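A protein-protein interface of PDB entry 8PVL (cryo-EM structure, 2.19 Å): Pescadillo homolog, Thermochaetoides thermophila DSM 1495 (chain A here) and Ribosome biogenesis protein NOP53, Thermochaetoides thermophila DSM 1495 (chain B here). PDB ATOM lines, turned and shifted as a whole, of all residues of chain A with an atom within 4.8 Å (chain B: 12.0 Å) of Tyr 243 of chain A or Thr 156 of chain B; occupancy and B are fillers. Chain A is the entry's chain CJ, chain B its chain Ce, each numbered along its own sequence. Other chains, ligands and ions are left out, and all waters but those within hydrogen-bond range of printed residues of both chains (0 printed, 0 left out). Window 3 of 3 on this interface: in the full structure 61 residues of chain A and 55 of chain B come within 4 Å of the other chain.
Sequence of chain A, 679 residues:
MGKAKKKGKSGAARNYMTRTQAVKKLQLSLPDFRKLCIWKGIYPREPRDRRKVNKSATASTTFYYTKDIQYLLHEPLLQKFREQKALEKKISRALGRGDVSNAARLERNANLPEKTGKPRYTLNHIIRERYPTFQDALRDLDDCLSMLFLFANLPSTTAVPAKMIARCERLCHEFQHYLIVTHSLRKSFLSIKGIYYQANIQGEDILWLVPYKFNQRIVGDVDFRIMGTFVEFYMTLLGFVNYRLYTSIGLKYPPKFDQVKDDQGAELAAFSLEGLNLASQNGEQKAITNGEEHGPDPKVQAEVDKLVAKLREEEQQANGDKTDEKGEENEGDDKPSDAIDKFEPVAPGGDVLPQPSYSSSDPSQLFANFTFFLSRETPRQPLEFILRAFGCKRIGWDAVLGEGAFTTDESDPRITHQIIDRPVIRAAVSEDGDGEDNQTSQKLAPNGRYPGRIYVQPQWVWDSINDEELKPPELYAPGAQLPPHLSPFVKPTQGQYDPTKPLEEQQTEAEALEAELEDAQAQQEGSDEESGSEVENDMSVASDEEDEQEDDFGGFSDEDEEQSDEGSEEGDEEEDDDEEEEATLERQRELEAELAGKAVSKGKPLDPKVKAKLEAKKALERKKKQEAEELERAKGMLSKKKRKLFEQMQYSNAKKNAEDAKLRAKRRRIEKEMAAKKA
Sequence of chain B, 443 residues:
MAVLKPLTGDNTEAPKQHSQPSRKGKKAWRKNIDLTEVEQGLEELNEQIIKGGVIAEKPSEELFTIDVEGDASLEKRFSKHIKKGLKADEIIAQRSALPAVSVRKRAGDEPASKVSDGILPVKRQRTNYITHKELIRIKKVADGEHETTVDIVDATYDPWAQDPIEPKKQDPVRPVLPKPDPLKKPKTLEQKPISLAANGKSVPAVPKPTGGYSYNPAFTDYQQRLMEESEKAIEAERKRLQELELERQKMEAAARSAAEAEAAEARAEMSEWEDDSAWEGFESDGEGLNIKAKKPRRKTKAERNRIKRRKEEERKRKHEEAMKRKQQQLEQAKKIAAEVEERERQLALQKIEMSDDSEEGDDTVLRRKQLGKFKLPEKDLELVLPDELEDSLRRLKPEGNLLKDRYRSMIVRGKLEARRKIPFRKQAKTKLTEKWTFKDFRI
Of the printed residues of chain B, Phe 240 of chain A touches Tyr 157, Pro 159 and Trp 160.
Tyr 243 of chain A touches just these residues of chain B: Thr 156 (3.5 Å) and Asp 158 (3.3 Å).
Of the printed residues of chain B, Arg 244 of chain A touches Trp 160.
No residue of chain B comes within 4 Å of Leu 245 of chain A.
Tyr 246 of chain A touches none of the printed residues of chain B.
No residue of chain B comes within 4 Å of Thr 247 of chain A.
Thr 156 of chain B touches one residue of chain A.
Of the printed residues of chain A, Trp 160 of chain B touches Phe 240 (3.9 Å), Val 241 (3.997 Å) and Arg 244 (3.6 Å).
The nearest residue of chain B that does not touch Tyr 243 of chain A is Tyr 157 of chain B (4.2 Å).
The nearest printed residue of chain A that does not touch Thr 156 of chain B is Phe 240 of chain A (5.6 Å).
The nearest printed residue of chain B that does not touch Arg 244 of chain A is Asp 158 of chain B (4.3 Å).
OG1 of Thr 247 of chain A lies within hydrogen-bond range of O of Tyr 243 of chain A.
Along chain A the printed residues that touch a printed residue of chain B span positions 240 to 244.
Among the printed residues, 7 pairs touch across the chains.
Among the printed residues, no Asp or Glu carboxylate lies within 4 Å of a Lys or Arg side-chain nitrogen of the other chain.
Phe 240 of chain A touches Tyr 157 of chain B (CE1 to O, 3.4 Å).
CD1 of Phe 240 of chain A touches CD of Pro 159 of chain B, at 3.6 Å.
Trp 160 of chain B touches Phe 240 of chain A.
Val 241 of chain A touches Trp 160 of chain B.
Tyr 243 of chain A touches Thr 156 of chain B.
Tyr 243 of chain A touches Asp 158 of chain B.
NH1 of Arg 244 of chain A touches O of Trp 160 of chain B (3.6 Å).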
ATOM      1  N   GLY A 239       0.913  -9.203  22.995  1.00  0.00           N
ATOM      2  CA  GLY A 239       0.447  -9.594  24.322  1.00  0.00           C
ATOM      3  C   GLY A 239      -0.025  -8.413  25.157  1.00  0.00           C
ATOM      4  O   GLY A 239      -1.118  -8.437  25.738  1.00  0.00           O
ATOM      5  N   PHE A 240       0.773  -7.344  25.187  1.00  0.00           N
ATOM      6  CA  PHE A 240       0.411  -6.162  25.963  1.00  0.00           C
ATOM      7  C   PHE A 240      -0.766  -5.424  25.341  1.00  0.00           C
ATOM      8  O   PHE A 240      -1.622  -4.893  26.064  1.00  0.00           O
ATOM      9  CB  PHE A 240       1.617  -5.235  26.089  1.00  0.00           C
ATOM     10  CG  PHE A 240       2.674  -5.748  27.014  1.00  0.00           C
ATOM     11  CD1 PHE A 240       2.361  -6.095  28.316  1.00  0.00           C
ATOM     12  CD2 PHE A 240       3.982  -5.889  26.582  1.00  0.00           C
ATOM     13  CE1 PHE A 240       3.332  -6.568  29.172  1.00  0.00           C
ATOM     14  CE2 PHE A 240       4.957  -6.365  27.433  1.00  0.00           C
ATOM     15  CZ  PHE A 240       4.629  -6.703  28.730  1.00  0.00           C
ATOM     16  N   VAL A 241      -0.827  -5.378  24.006  1.00  0.00           N
ATOM     17  CA  VAL A 241      -1.954  -4.732  23.334  1.00  0.00           C
ATOM     18  C   VAL A 241      -3.255  -5.467  23.645  1.00  0.00           C
ATOM     19  O   VAL A 241      -4.285  -4.843  23.943  1.00  0.00           O
ATOM     20  CB  VAL A 241      -1.683  -4.645  21.819  1.00  0.00           C
ATOM     21  CG1 VAL A 241      -2.961  -4.387  21.038  1.00  0.00           C
ATOM     22  CG2 VAL A 241      -0.663  -3.561  21.532  1.00  0.00           C
ATOM     23  N   ASN A 242      -3.215  -6.803  23.616  1.00  0.00           N
ATOM     24  CA  ASN A 242      -4.383  -7.609  23.953  1.00  0.00           C
ATOM     25  C   ASN A 242      -4.814  -7.391  25.396  1.00  0.00           C
ATOM     26  O   ASN A 242      -6.013  -7.267  25.677  1.00  0.00           O
ATOM     27  CB  ASN A 242      -4.083  -9.087  23.712  1.00  0.00           C
ATOM     28  CG  ASN A 242      -4.312  -9.505  22.281  1.00  0.00           C
ATOM     29  OD1 ASN A 242      -4.790  -8.724  21.462  1.00  0.00           O
ATOM     30  ND2 ASN A 242      -3.975 -10.749  21.969  1.00  0.00           N
ATOM     31  N   TYR A 243      -3.849  -7.340  26.325  1.00  0.00           N
ATOM     32  CA  TYR A 243      -4.193  -7.093  27.725  1.00  0.00           C
ATOM     33  C   TYR A 243      -4.856  -5.733  27.905  1.00  0.00           C
ATOM     34  O   TYR A 243      -5.858  -5.615  28.622  1.00  0.00           O
ATOM     35  CB  TYR A 243      -2.952  -7.191  28.612  1.00  0.00           C
ATOM     36  CG  TYR A 243      -3.234  -6.874  30.067  1.00  0.00           C
ATOM     37  CD1 TYR A 243      -3.816  -7.819  30.900  1.00  0.00           C
ATOM     38  CD2 TYR A 243      -2.922  -5.629  30.606  1.00  0.00           C
ATOM     39  CE1 TYR A 243      -4.082  -7.536  32.223  1.00  0.00           C
ATOM     40  CE2 TYR A 243      -3.187  -5.339  31.928  1.00  0.00           C
ATOM     41  CZ  TYR A 243      -3.764  -6.296  32.732  1.00  0.00           C
ATOM     42  OH  TYR A 243      -4.027  -6.012  34.052  1.00  0.00           O
ATOM     43  N   ARG A 244      -4.316  -4.699  27.253  1.00  0.00           N
ATOM     44  CA  ARG A 244      -4.878  -3.358  27.392  1.00  0.00           C
ATOM     45  C   ARG A 244      -6.288  -3.282  26.817  1.00  0.00           C
ATOM     46  O   ARG A 244      -7.179  -2.683  27.429  1.00  0.00           O
ATOM     47  CB  ARG A 244      -3.963  -2.333  26.722  1.00  0.00           C
ATOM     48  CG  ARG A 244      -4.593  -0.966  26.529  1.00  0.00           C
ATOM     49  CD  ARG A 244      -3.923   0.086  27.391  1.00  0.00           C
ATOM     50  NE  ARG A 244      -4.286   1.435  26.977  1.00  0.00           N
ATOM     51  CZ  ARG A 244      -3.909   2.537  27.608  1.00  0.00           C
ATOM     52  NH1 ARG A 244      -3.159   2.487  28.696  1.00  0.00           N
ATOM     53  NH2 ARG A 244      -4.293   3.720  27.136  1.00  0.00           N
ATOM     54  N   LEU A 245      -6.521  -3.908  25.658  1.00  0.00           N
ATOM     55  CA  LEU A 245      -7.855  -3.869  25.058  1.00  0.00           C
ATOM     56  C   LEU A 245      -8.875  -4.644  25.891  1.00  0.00           C
ATOM     57  O   LEU A 245     -10.015  -4.185  26.075  1.00  0.00           O
ATOM     58  CB  LEU A 245      -7.799  -4.408  23.630  1.00  0.00           C
ATOM     59  CG  LEU A 245      -7.035  -3.525  22.641  1.00  0.00           C
ATOM     60  CD1 LEU A 245      -6.862  -4.225  21.308  1.00  0.00           C
ATOM     61  CD2 LEU A 245      -7.740  -2.195  22.461  1.00  0.00           C
ATOM     62  N   TYR A 246      -8.483  -5.815  26.408  1.00  0.00           N
ATOM     63  CA  TYR A 246      -9.389  -6.595  27.246  1.00  0.00           C
ATOM     64  C   TYR A 246      -9.721  -5.858  28.539  1.00  0.00           C
ATOM     65  O   TYR A 246     -10.875  -5.861  28.984  1.00  0.00           O
ATOM     66  CB  TYR A 246      -8.778  -7.959  27.554  1.00  0.00           C
ATOM     67  CG  TYR A 246      -9.076  -9.025  26.526  1.00  0.00           C
ATOM     68  CD1 TYR A 246      -8.665  -8.884  25.208  1.00  0.00           C
ATOM     69  CD2 TYR A 246      -9.763 -10.176  26.875  1.00  0.00           C
ATOM     70  CE1 TYR A 246      -8.929  -9.856  24.269  1.00  0.00           C
ATOM     71  CE2 TYR A 246     -10.034 -11.152  25.943  1.00  0.00           C
ATOM     72  CZ  TYR A 246      -9.614 -10.989  24.642  1.00  0.00           C
ATOM     73  OH  TYR A 246      -9.880 -11.961  23.709  1.00  0.00           O
ATOM     74  N   THR A 247      -8.726  -5.207  29.149  1.00  0.00           N
ATOM     75  CA  THR A 247      -8.993  -4.429  30.353  1.00  0.00           C
ATOM     76  C   THR A 247      -9.831  -3.192  30.051  1.00  0.00           C
ATOM     77  O   THR A 247     -10.619  -2.758  30.898  1.00  0.00           O
ATOM     78  CB  THR A 247      -7.676  -4.032  31.020  1.00  0.00           C
ATOM     79  OG1 THR A 247      -6.761  -5.133  30.954  1.00  0.00           O
ATOM     80  CG2 THR A 247      -7.902  -3.667  32.477  1.00  0.00           C
ATOM     81  N   TYR A 253      -7.878 -11.023  31.334  1.00  0.00           N
ATOM     82  CA  TYR A 253      -6.874 -11.441  30.377  1.00  0.00           C
ATOM     83  C   TYR A 253      -5.780 -12.213  31.101  1.00  0.00           C
ATOM     84  O   TYR A 253      -5.352 -11.805  32.186  1.00  0.00           O
ATOM     85  CB  TYR A 253      -6.270 -10.235  29.642  1.00  0.00           C
ATOM     86  CG  TYR A 253      -5.363 -10.627  28.504  1.00  0.00           C
ATOM     87  CD1 TYR A 253      -5.889 -10.996  27.276  1.00  0.00           C
ATOM     88  CD2 TYR A 253      -3.985 -10.649  28.664  1.00  0.00           C
ATOM     89  CE1 TYR A 253      -5.069 -11.368  26.236  1.00  0.00           C
ATOM     90  CE2 TYR A 253      -3.156 -11.016  27.629  1.00  0.00           C
ATOM     91  CZ  TYR A 253      -3.703 -11.375  26.416  1.00  0.00           C
ATOM     92  OH  TYR A 253      -2.879 -11.742  25.379  1.00  0.00           O
ATOM     93  N   THR B 156       0.990  -8.642  37.059  1.00  0.00           N
ATOM     94  CA  THR B 156       1.194  -8.456  35.629  1.00  0.00           C
ATOM     95  C   THR B 156       1.875  -7.122  35.330  1.00  0.00           C
ATOM     96  O   THR B 156       2.356  -6.442  36.237  1.00  0.00           O
ATOM     97  CB  THR B 156      -0.133  -8.523  34.857  1.00  0.00           C
ATOM     98  OG1 THR B 156       0.106  -8.241  33.472  1.00  0.00           O
ATOM     99  CG2 THR B 156      -1.121  -7.510  35.413  1.00  0.00           C
ATOM    100  N   TYR B 157       1.919  -6.762  34.048  1.00  0.00           N
ATOM    101  CA  TYR B 157       2.568  -5.542  33.590  1.00  0.00           C
ATOM    102  C   TYR B 157       1.643  -4.920  32.554  1.00  0.00           C
ATOM    103  O   TYR B 157       1.192  -5.597  31.625  1.00  0.00           O
ATOM    104  CB  TYR B 157       3.962  -5.858  32.999  1.00  0.00           C
ATOM    105  CG  TYR B 157       4.866  -4.703  32.546  1.00  0.00           C
ATOM    106  CD1 TYR B 157       4.467  -3.371  32.601  1.00  0.00           C
ATOM    107  CD2 TYR B 157       6.137  -4.971  32.056  1.00  0.00           C
ATOM    108  CE1 TYR B 157       5.299  -2.352  32.183  1.00  0.00           C
ATOM    109  CE2 TYR B 157       6.975  -3.956  31.640  1.00  0.00           C
ATOM    110  CZ  TYR B 157       6.550  -2.651  31.703  1.00  0.00           C
ATOM    111  OH  TYR B 157       7.377  -1.635  31.291  1.00  0.00           O
ATOM    112  N   ASP B 158       1.352  -3.633  32.726  1.00  0.00           N
ATOM    113  CA  ASP B 158       0.523  -2.894  31.780  1.00  0.00           C
ATOM    114  C   ASP B 158       1.325  -1.627  31.490  1.00  0.00           C
ATOM    115  O   ASP B 158       1.289  -0.667  32.276  1.00  0.00           O
ATOM    116  CB  ASP B 158      -0.865  -2.626  32.371  1.00  0.00           C
ATOM    117  CG  ASP B 158      -1.795  -1.804  31.460  1.00  0.00           C
ATOM    118  OD1 ASP B 158      -3.013  -2.092  31.460  1.00  0.00           O
ATOM    119  OD2 ASP B 158      -1.366  -0.867  30.772  1.00  0.00           O
ATOM    120  N   PRO B 159       2.067  -1.588  30.367  1.00  0.00           N
ATOM    121  CA  PRO B 159       2.814  -0.372  30.013  1.00  0.00           C
ATOM    122  C   PRO B 159       1.895   0.723  29.497  1.00  0.00           C
ATOM    123  O   PRO B 159       0.674   0.554  29.518  1.00  0.00           O
ATOM    124  CB  PRO B 159       3.787  -0.860  28.935  1.00  0.00           C
ATOM    125  CG  PRO B 159       3.095  -2.016  28.312  1.00  0.00           C
ATOM    126  CD  PRO B 159       2.309  -2.681  29.410  1.00  0.00           C
ATOM    127  N   TRP B 160       2.469   1.841  29.042  1.00  0.00           N
ATOM    128  CA  TRP B 160       1.736   3.049  28.651  1.00  0.00           C
ATOM    129  C   TRP B 160       0.899   3.610  29.799  1.00  0.00           C
ATOM    130  O   TRP B 160      -0.147   4.224  29.567  1.00  0.00           O
ATOM    131  CB  TRP B 160       0.838   2.815  27.426  1.00  0.00           C
ATOM    132  CG  TRP B 160       1.495   2.108  26.291  1.00  0.00           C
ATOM    133  CD1 TRP B 160       2.466   2.598  25.475  1.00  0.00           C
ATOM    134  CD2 TRP B 160       1.231   0.773  25.844  1.00  0.00           C
ATOM    135  NE1 TRP B 160       2.821   1.655  24.543  1.00  0.00           N
ATOM    136  CE2 TRP B 160       2.076   0.525  24.748  1.00  0.00           C
ATOM    137  CE3 TRP B 160       0.359  -0.235  26.264  1.00  0.00           C
ATOM    138  CZ2 TRP B 160       2.077  -0.689  24.068  1.00  0.00           C
ATOM    139  CZ3 TRP B 160       0.362  -1.439  25.587  1.00  0.00           C
ATOM    140  CH2 TRP B 160       1.215  -1.656  24.502  1.00  0.00           C
ATOM    141  N   ALA B 161       1.342   3.413  31.036  1.00  0.00           N
ATOM    142  CA  ALA B 161       0.581   3.844  32.202  1.00  0.00           C
ATOM    143  C   ALA B 161       1.504   4.390  33.284  1.00  0.00           C
ATOM    144  O   ALA B 161       2.509   3.769  33.626  1.00  0.00           O
ATOM    145  CB  ALA B 161      -0.249   2.692  32.747  1.00  0.00           C
